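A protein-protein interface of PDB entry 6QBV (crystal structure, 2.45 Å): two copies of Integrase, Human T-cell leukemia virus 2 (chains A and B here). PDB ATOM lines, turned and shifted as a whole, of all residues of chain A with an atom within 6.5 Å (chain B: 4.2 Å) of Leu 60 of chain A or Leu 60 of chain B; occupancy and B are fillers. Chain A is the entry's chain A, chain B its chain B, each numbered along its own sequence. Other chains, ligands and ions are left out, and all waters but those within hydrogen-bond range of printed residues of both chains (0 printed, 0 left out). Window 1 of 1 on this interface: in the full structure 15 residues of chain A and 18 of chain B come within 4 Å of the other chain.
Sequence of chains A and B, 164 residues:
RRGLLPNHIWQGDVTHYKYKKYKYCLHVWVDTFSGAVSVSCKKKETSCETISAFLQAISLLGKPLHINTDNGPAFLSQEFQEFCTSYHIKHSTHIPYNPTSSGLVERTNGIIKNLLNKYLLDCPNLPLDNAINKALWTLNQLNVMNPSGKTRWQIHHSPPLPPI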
ATOM      1  N   VAL A  37      11.803 -19.245   1.512  1.00  0.00           N
ATOM      2  CA  VAL A  37      12.768 -19.340   0.425  1.00  0.00           C
ATOM      3  C   VAL A  37      12.890 -17.990  -0.280  1.00  0.00           C
ATOM      4  O   VAL A  37      11.898 -17.314  -0.456  1.00  0.00           O
ATOM      5  CB  VAL A  37      12.323 -20.438  -0.571  1.00  0.00           C
ATOM      6  CG1 VAL A  37      13.400 -20.711  -1.609  1.00  0.00           C
ATOM      7  CG2 VAL A  37      12.041 -21.721   0.165  1.00  0.00           C
ATOM      8  N   SER A  38      14.087 -17.638  -0.744  1.00  0.00           N
ATOM      9  CA  SER A  38      14.264 -16.584  -1.743  1.00  0.00           C
ATOM     10  C   SER A  38      15.026 -17.145  -2.939  1.00  0.00           C
ATOM     11  O   SER A  38      16.004 -17.844  -2.759  1.00  0.00           O
ATOM     12  CB  SER A  38      15.040 -15.399  -1.200  1.00  0.00           C
ATOM     13  OG  SER A  38      15.470 -14.528  -2.251  1.00  0.00           O
ATOM     14  N   VAL A  39      14.605 -16.774  -4.142  1.00  0.00           N
ATOM     15  CA  VAL A  39      15.213 -17.242  -5.365  1.00  0.00           C
ATOM     16  C   VAL A  39      15.371 -16.018  -6.239  1.00  0.00           C
ATOM     17  O   VAL A  39      14.408 -15.262  -6.390  1.00  0.00           O
ATOM     18  CB  VAL A  39      14.341 -18.287  -6.093  1.00  0.00           C
ATOM     19  CG1 VAL A  39      15.021 -18.717  -7.374  1.00  0.00           C
ATOM     20  CG2 VAL A  39      14.062 -19.507  -5.220  1.00  0.00           C
ATOM     21  N   LEU A  55      21.044  -9.553  -1.388  1.00  0.00           N
ATOM     22  CA  LEU A  55      20.314  -8.342  -1.008  1.00  0.00           C
ATOM     23  C   LEU A  55      18.810  -8.476  -1.299  1.00  0.00           C
ATOM     24  O   LEU A  55      17.968  -8.125  -0.468  1.00  0.00           O
ATOM     25  CB  LEU A  55      20.947  -7.106  -1.676  1.00  0.00           C
ATOM     26  CG  LEU A  55      22.214  -6.548  -1.016  1.00  0.00           C
ATOM     27  CD1 LEU A  55      22.816  -5.439  -1.871  1.00  0.00           C
ATOM     28  CD2 LEU A  55      21.881  -5.979   0.369  1.00  0.00           C
ATOM     29  N   GLN A  56      18.458  -9.050  -2.453  1.00  0.00           N
ATOM     30  CA  GLN A  56      17.068  -9.393  -2.740  1.00  0.00           C
ATOM     31  C   GLN A  56      16.504 -10.332  -1.667  1.00  0.00           C
ATOM     32  O   GLN A  56      15.382 -10.143  -1.223  1.00  0.00           O
ATOM     33  CB  GLN A  56      16.946  -9.969  -4.149  1.00  0.00           C
ATOM     34  CG  GLN A  56      15.525 -10.055  -4.677  1.00  0.00           C
ATOM     35  CD  GLN A  56      15.470 -10.637  -6.073  1.00  0.00           C
ATOM     36  OE1 GLN A  56      16.487 -10.884  -6.713  1.00  0.00           O
ATOM     37  NE2 GLN A  56      14.264 -10.865  -6.563  1.00  0.00           N
ATOM     38  N   ALA A  57      17.301 -11.302  -1.194  1.00  0.00           N
ATOM     39  CA  ALA A  57      16.799 -12.261  -0.220  1.00  0.00           C
ATOM     40  C   ALA A  57      16.531 -11.544   1.105  1.00  0.00           C
ATOM     41  O   ALA A  57      15.605 -11.913   1.842  1.00  0.00           O
ATOM     42  CB  ALA A  57      17.760 -13.448  -0.057  1.00  0.00           C
ATOM     43  N   ILE A  58      17.389 -10.555   1.408  1.00  0.00           N
ATOM     44  CA  ILE A  58      17.340  -9.871   2.690  1.00  0.00           C
ATOM     45  C   ILE A  58      16.091  -8.993   2.677  1.00  0.00           C
ATOM     46  O   ILE A  58      15.325  -8.887   3.654  1.00  0.00           O
ATOM     47  CB  ILE A  58      18.637  -9.073   2.982  1.00  0.00           C
ATOM     48  CG1 ILE A  58      19.753 -10.026   3.422  1.00  0.00           C
ATOM     49  CG2 ILE A  58      18.400  -7.967   4.026  1.00  0.00           C
ATOM     50  CD1 ILE A  58      21.162  -9.454   3.330  1.00  0.00           C
ATOM     51  N   SER A  59      15.893  -8.372   1.524  1.00  0.00           N
ATOM     52  CA  SER A  59      14.666  -7.608   1.381  1.00  0.00           C
ATOM     53  C   SER A  59      13.453  -8.537   1.484  1.00  0.00           C
ATOM     54  O   SER A  59      12.460  -8.136   2.061  1.00  0.00           O
ATOM     55  CB  SER A  59      14.676  -6.822   0.133  1.00  0.00           C
ATOM     56  OG  SER A  59      13.379  -6.817  -0.438  1.00  0.00           O
ATOM     57  N   LEU A  60      13.516  -9.778   0.959  1.00  0.00           N
ATOM     58  CA  LEU A  60      12.353 -10.662   1.070  1.00  0.00           C
ATOM     59  C   LEU A  60      12.211 -11.209   2.491  1.00  0.00           C
ATOM     60  O   LEU A  60      11.102 -11.252   3.019  1.00  0.00           O
ATOM     61  CB  LEU A  60      12.376 -11.801   0.043  1.00  0.00           C
ATOM     62  CG  LEU A  60      11.075 -12.615  -0.017  1.00  0.00           C
ATOM     63  CD1 LEU A  60       9.965 -11.901  -0.823  1.00  0.00           C
ATOM     64  CD2 LEU A  60      11.319 -13.980  -0.634  1.00  0.00           C
ATOM     65  N   LEU A  61      13.330 -11.588   3.118  1.00  0.00           N
ATOM     66  CA  LEU A  61      13.249 -12.512   4.229  1.00  0.00           C
ATOM     67  C   LEU A  61      13.589 -11.833   5.545  1.00  0.00           C
ATOM     68  O   LEU A  61      13.259 -12.381   6.608  1.00  0.00           O
ATOM     69  CB  LEU A  61      14.184 -13.689   3.956  1.00  0.00           C
ATOM     70  CG  LEU A  61      13.689 -14.674   2.915  1.00  0.00           C
ATOM     71  CD1 LEU A  61      14.623 -15.872   2.875  1.00  0.00           C
ATOM     72  CD2 LEU A  61      12.246 -15.098   3.225  1.00  0.00           C
ATOM     73  N   GLY A  62      14.292 -10.691   5.467  1.00  0.00           N
ATOM     74  CA  GLY A  62      15.007 -10.213   6.653  1.00  0.00           C
ATOM     75  C   GLY A  62      16.510 -10.527   6.631  1.00  0.00           C
ATOM     76  O   GLY A  62      17.032 -11.181   5.705  1.00  0.00           O
ATOM     77  N   ASN A 133       8.449 -15.875  -9.496  1.00  0.00           N
ATOM     78  CA  ASN A 133       7.702 -15.144  -8.478  1.00  0.00           C
ATOM     79  C   ASN A 133       6.393 -15.833  -8.128  1.00  0.00           C
ATOM     80  O   ASN A 133       5.967 -15.774  -6.973  1.00  0.00           O
ATOM     81  CB  ASN A 133       7.449 -13.687  -8.866  1.00  0.00           C
ATOM     82  CG  ASN A 133       8.707 -12.867  -8.704  1.00  0.00           C
ATOM     83  OD1 ASN A 133       9.190 -12.273  -9.664  1.00  0.00           O
ATOM     84  ND2 ASN A 133       9.235 -12.826  -7.493  1.00  0.00           N
ATOM     85  N   LEU A 136       7.569 -18.697  -5.733  1.00  0.00           N
ATOM     86  CA  LEU A 136       7.884 -18.162  -4.417  1.00  0.00           C
ATOM     87  C   LEU A 136       6.607 -17.932  -3.617  1.00  0.00           C
ATOM     88  O   LEU A 136       6.470 -18.388  -2.479  1.00  0.00           O
ATOM     89  CB  LEU A 136       8.686 -16.870  -4.616  1.00  0.00           C
ATOM     90  CG  LEU A 136      10.130 -17.107  -5.060  1.00  0.00           C
ATOM     91  CD1 LEU A 136      10.948 -15.817  -5.131  1.00  0.00           C
ATOM     92  CD2 LEU A 136      10.784 -18.155  -4.160  1.00  0.00           C
ATOM     93  N   ASN A 140       5.925 -20.096  -0.480  1.00  0.00           N
ATOM     94  CA  ASN A 140       6.044 -19.475   0.833  1.00  0.00           C
ATOM     95  C   ASN A 140       4.674 -19.291   1.478  1.00  0.00           C
ATOM     96  O   ASN A 140       4.529 -19.537   2.672  1.00  0.00           O
ATOM     97  CB  ASN A 140       6.810 -18.158   0.808  1.00  0.00           C
ATOM     98  CG  ASN A 140       8.303 -18.320   0.643  1.00  0.00           C
ATOM     99  OD1 ASN A 140       8.916 -19.156   1.296  1.00  0.00           O
ATOM    100  ND2 ASN A 140       8.916 -17.484  -0.183  1.00  0.00           N
ATOM    101  N   GLN A 141       3.672 -18.851   0.703  1.00  0.00           N
ATOM    102  CA  GLN A 141       2.477 -18.278   1.309  1.00  0.00           C
ATOM    103  C   GLN A 141       1.250 -19.153   1.087  1.00  0.00           C
ATOM    104  O   GLN A 141       0.278 -19.021   1.827  1.00  0.00           O
ATOM    105  CB  GLN A 141       2.246 -16.849   0.814  1.00  0.00           C
ATOM    106  CG  GLN A 141       3.487 -15.970   0.918  1.00  0.00           C
ATOM    107  CD  GLN A 141       3.224 -14.567   0.417  1.00  0.00           C
ATOM    108  OE1 GLN A 141       2.190 -13.960   0.712  1.00  0.00           O
ATOM    109  NE2 GLN A 141       4.160 -14.037  -0.353  1.00  0.00           N
ATOM    110  N   TRP A 153       5.671 -18.873   5.435  1.00  0.00           N
ATOM    111  CA  TRP A 153       5.578 -17.445   5.692  1.00  0.00           C
ATOM    112  C   TRP A 153       5.071 -17.203   7.106  1.00  0.00           C
ATOM    113  O   TRP A 153       5.555 -16.311   7.788  1.00  0.00           O
ATOM    114  CB  TRP A 153       4.608 -16.786   4.719  1.00  0.00           C
ATOM    115  CG  TRP A 153       4.970 -15.397   4.298  1.00  0.00           C
ATOM    116  CD1 TRP A 153       4.169 -14.301   4.375  1.00  0.00           C
ATOM    117  CD2 TRP A 153       6.191 -14.957   3.665  1.00  0.00           C
ATOM    118  NE1 TRP A 153       4.803 -13.218   3.821  1.00  0.00           N
ATOM    119  CE2 TRP A 153       6.039 -13.584   3.378  1.00  0.00           C
ATOM    120  CE3 TRP A 153       7.363 -15.592   3.250  1.00  0.00           C
ATOM    121  CZ2 TRP A 153       7.026 -12.832   2.748  1.00  0.00           C
ATOM    122  CZ3 TRP A 153       8.327 -14.860   2.598  1.00  0.00           C
ATOM    123  CH2 TRP A 153       8.169 -13.496   2.362  1.00  0.00           C
ATOM    124  N   HIS A 156       7.713 -17.993   9.505  1.00  0.00           N
ATOM    125  CA  HIS A 156       8.789 -17.023   9.358  1.00  0.00           C
ATOM    126  C   HIS A 156       8.450 -15.710  10.067  1.00  0.00           C
ATOM    127  O   HIS A 156       9.368 -15.001  10.452  1.00  0.00           O
ATOM    128  CB  HIS A 156       9.141 -16.791   7.881  1.00  0.00           C
ATOM    129  CG  HIS A 156      10.479 -16.174   7.699  1.00  0.00           C
ATOM    130  ND1 HIS A 156      11.681 -16.914   7.884  1.00  0.00           N
ATOM    131  CD2 HIS A 156      10.825 -14.898   7.379  1.00  0.00           C
ATOM    132  CE1 HIS A 156      12.711 -16.091   7.698  1.00  0.00           C
ATOM    133  NE2 HIS A 156      12.207 -14.839   7.364  1.00  0.00           N
ATOM    134  N   HIS A 157       7.151 -15.381  10.214  1.00  0.00           N
ATOM    135  CA  HIS A 157       6.713 -14.060  10.648  1.00  0.00           C
ATOM    136  C   HIS A 157       6.036 -14.161  12.015  1.00  0.00           C
ATOM    137  O   HIS A 157       5.481 -13.190  12.502  1.00  0.00           O
ATOM    138  CB  HIS A 157       5.859 -13.323   9.581  1.00  0.00           C
ATOM    139  CG  HIS A 157       6.567 -12.973   8.315  1.00  0.00           C
ATOM    140  ND1 HIS A 157       7.441 -11.904   8.218  1.00  0.00           N
ATOM    141  CD2 HIS A 157       6.556 -13.546   7.093  1.00  0.00           C
ATOM    142  CE1 HIS A 157       7.968 -11.850   7.002  1.00  0.00           C
ATOM    143  NE2 HIS A 157       7.429 -12.842   6.290  1.00  0.00           N
ATOM    144  N   VAL B  37       6.009  -1.495   1.424  1.00  0.00           N
ATOM    145  CA  VAL B  37       6.206  -1.063   0.038  1.00  0.00           C
ATOM    146  C   VAL B  37       6.983  -2.107  -0.771  1.00  0.00           C
ATOM    147  O   VAL B  37       7.933  -2.736  -0.284  1.00  0.00           O
ATOM    148  CB  VAL B  37       6.932   0.298  -0.027  1.00  0.00           C
ATOM    149  CG1 VAL B  37       8.264   0.275   0.733  1.00  0.00           C
ATOM    150  CG2 VAL B  37       7.139   0.792  -1.464  1.00  0.00           C
ATOM    151  N   SER B  38       6.604  -2.217  -2.049  1.00  0.00           N
ATOM    152  CA  SER B  38       7.371  -2.965  -3.031  1.00  0.00           C
ATOM    153  C   SER B  38       7.792  -2.017  -4.154  1.00  0.00           C
ATOM    154  O   SER B  38       6.962  -1.277  -4.659  1.00  0.00           O
ATOM    155  CB  SER B  38       6.548  -4.144  -3.579  1.00  0.00           C
ATOM    156  OG  SER B  38       7.176  -4.725  -4.731  1.00  0.00           O
ATOM    157  N   GLN B  56       6.139  -9.551  -8.605  1.00  0.00           N
ATOM    158  CA  GLN B  56       7.208  -9.413  -7.629  1.00  0.00           C
ATOM    159  C   GLN B  56       6.681  -8.833  -6.308  1.00  0.00           C
ATOM    160  O   GLN B  56       7.048  -9.319  -5.228  1.00  0.00           O
ATOM    161  CB  GLN B  56       8.335  -8.601  -8.232  1.00  0.00           C
ATOM    162  CG  GLN B  56       9.654  -8.695  -7.475  1.00  0.00           C
ATOM    163  CD  GLN B  56      10.597  -7.630  -7.975  1.00  0.00           C
ATOM    164  OE1 GLN B  56      10.574  -7.250  -9.153  1.00  0.00           O
ATOM    165  NE2 GLN B  56      11.394  -7.099  -7.066  1.00  0.00           N
ATOM    166  N   ALA B  57       5.781  -7.835  -6.406  1.00  0.00           N
ATOM    167  CA  ALA B  57       5.186  -7.225  -5.231  1.00  0.00           C
ATOM    168  C   ALA B  57       4.390  -8.285  -4.468  1.00  0.00           C
ATOM    169  O   ALA B  57       4.399  -8.302  -3.240  1.00  0.00           O
ATOM    170  CB  ALA B  57       4.348  -6.033  -5.645  1.00  0.00           C
ATOM    171  N   ILE B  58       3.695  -9.178  -5.192  1.00  0.00           N
ATOM    172  CA  ILE B  58       2.886 -10.224  -4.561  1.00  0.00           C
ATOM    173  C   ILE B  58       3.789 -11.212  -3.821  1.00  0.00           C
ATOM    174  O   ILE B  58       3.449 -11.651  -2.741  1.00  0.00           O
ATOM    175  CB  ILE B  58       1.932 -10.921  -5.563  1.00  0.00           C
ATOM    176  CG1 ILE B  58       0.805  -9.985  -6.002  1.00  0.00           C
ATOM    177  CG2 ILE B  58       1.350 -12.196  -4.966  1.00  0.00           C
ATOM    178  CD1 ILE B  58       0.100 -10.423  -7.254  1.00  0.00           C
ATOM    179  N   SER B  59       4.959 -11.532  -4.374  1.00  0.00           N
ATOM    180  CA  SER B  59       5.900 -12.388  -3.662  1.00  0.00           C
ATOM    181  C   SER B  59       6.355 -11.664  -2.395  1.00  0.00           C
ATOM    182  O   SER B  59       6.578 -12.305  -1.385  1.00  0.00           O
ATOM    183  CB  SER B  59       7.121 -12.864  -4.517  1.00  0.00           C
ATOM    184  N   LEU B  60       6.495 -10.325  -2.434  1.00  0.00           N
ATOM    185  CA  LEU B  60       7.006  -9.582  -1.279  1.00  0.00           C
ATOM    186  C   LEU B  60       5.939  -9.405  -0.205  1.00  0.00           C
ATOM    187  O   LEU B  60       6.230  -9.641   0.961  1.00  0.00           O
ATOM    188  CB  LEU B  60       7.590  -8.237  -1.724  1.00  0.00           C
ATOM    189  CG  LEU B  60       8.392  -7.493  -0.653  1.00  0.00           C
ATOM    190  CD1 LEU B  60       9.774  -8.132  -0.444  1.00  0.00           C
ATOM    191  CD2 LEU B  60       8.553  -6.027  -1.013  1.00  0.00           C
ATOM    192  N   LEU B  61       4.701  -9.026  -0.602  1.00  0.00           N
ATOM    193  CA  LEU B  61       3.711  -8.495   0.335  1.00  0.00           C
ATOM    194  C   LEU B  61       2.563  -9.470   0.542  1.00  0.00           C
ATOM    195  O   LEU B  61       1.826  -9.337   1.510  1.00  0.00           O
ATOM    196  CB  LEU B  61       3.176  -7.130  -0.134  1.00  0.00           C
ATOM    197  CG  LEU B  61       4.224  -6.026  -0.342  1.00  0.00           C
ATOM    198  CD1 LEU B  61       3.648  -4.877  -1.166  1.00  0.00           C
ATOM    199  CD2 LEU B  61       4.740  -5.523   0.991  1.00  0.00           C
ATOM    200  N   GLY B  62       2.388 -10.432  -0.375  1.00  0.00           N
ATOM    201  CA  GLY B  62       1.136 -11.150  -0.372  1.00  0.00           C
ATOM    202  C   GLY B  62       0.155 -10.612  -1.418  1.00  0.00           C
ATOM    203  O   GLY B  62       0.440  -9.606  -2.073  1.00  0.00           O
ATOM    204  N   TRP B 153       6.928  -3.597   8.263  1.00  0.00           N
ATOM    205  CA  TRP B 153       6.980  -5.058   8.160  1.00  0.00           C
ATOM    206  C   TRP B 153       6.237  -5.733   9.306  1.00  0.00           C
ATOM    207  O   TRP B 153       5.558  -6.731   9.118  1.00  0.00           O
ATOM    208  CB  TRP B 153       8.416  -5.557   8.187  1.00  0.00           C
ATOM    209  CG  TRP B 153       8.685  -6.698   7.254  1.00  0.00           C
ATOM    210  CD1 TRP B 153       9.210  -7.908   7.591  1.00  0.00           C
ATOM    211  CD2 TRP B 153       8.492  -6.739   5.832  1.00  0.00           C
ATOM    212  NE1 TRP B 153       9.382  -8.685   6.484  1.00  0.00           N
ATOM    213  CE2 TRP B 153       8.956  -7.997   5.388  1.00  0.00           C
ATOM    214  CE3 TRP B 153       8.006  -5.837   4.877  1.00  0.00           C
ATOM    215  CZ2 TRP B 153       8.922  -8.384   4.048  1.00  0.00           C
ATOM    216  CZ3 TRP B 153       7.992  -6.211   3.545  1.00  0.00           C
ATOM    217  CH2 TRP B 153       8.424  -7.477   3.139  1.00  0.00           C
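The side-chain amide nitrogen (NE2) of Gln 141 of chain A sits at hydrogen-bond distance from the backbone carbonyl oxygen (O) of Ile 58 of chain B, at 3.4 Å.
The side-chain amide nitrogen (NE2) of Gln 141 of chain A is in hydrogen-bond range of the backbone carbonyl oxygen (O) of Ser 59 of chain B (3.1 Å).
The backbone carbonyl oxygen (O) of Asn 140 of chain A lies within hydrogen-bond range of the backbone NH (N) of Trp 153 of chain A (3.1 Å).
Among the printed residues, pairs that only touch across the chains: Gln 141 of chain A with Gly 62 of chain B, Leu 60 of chain A with Ser 59 of chain B, His 157 of chain A with Trp 153 of chain B, Asn 133 of chain A with Ser 59 of chain B, Ser 59 of chain A with Leu 60 of chain B, Trp 153 of chain A with Leu 60 of chain B, Leu 60 of chain A with Trp 153 of chain B, Leu 60 of chain A with Leu 60 of chain B and Asn 133 of chain A with Gln 56 of chain B.
Along chain B the printed residues that touch a printed residue of chain A span positions 56 to 153.
Of the 18 printed residues of chain A, 6 touch a printed residue of chain B.
Hydrophobic or aromatic side chains of chain A that line the printed part of chain B: Leu 60, Trp 153 and His 157.
Among the printed residues, 11 pairs touch across the chains.
Ser 59 of chain A touches Leu 60 of chain B, and with the chains exchanged Leu 60 of chain A touches Ser 59 of chain B.
Leu 60 of chain B touches its own counterpart, Leu 60 of chain A.
Leu 60 of chain A touches Trp 153 of chain B, and with the chains exchanged Trp 153 of chain A touches Leu 60 of chain B.
Of the 11 pairs that touch across the chains among the printed residues, 5 have their exchanged pair printed and touching as well.
Of the printed residues of chain B, His 157 of chain A touches Trp 153.
Of the printed residues of chain A, Ile 58 of chain B touches Gln 141 (3.4 Å).
Of chain A, only Ser 59, Leu 60 and Trp 153 come within 4 Å of Leu 60 of chain B.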
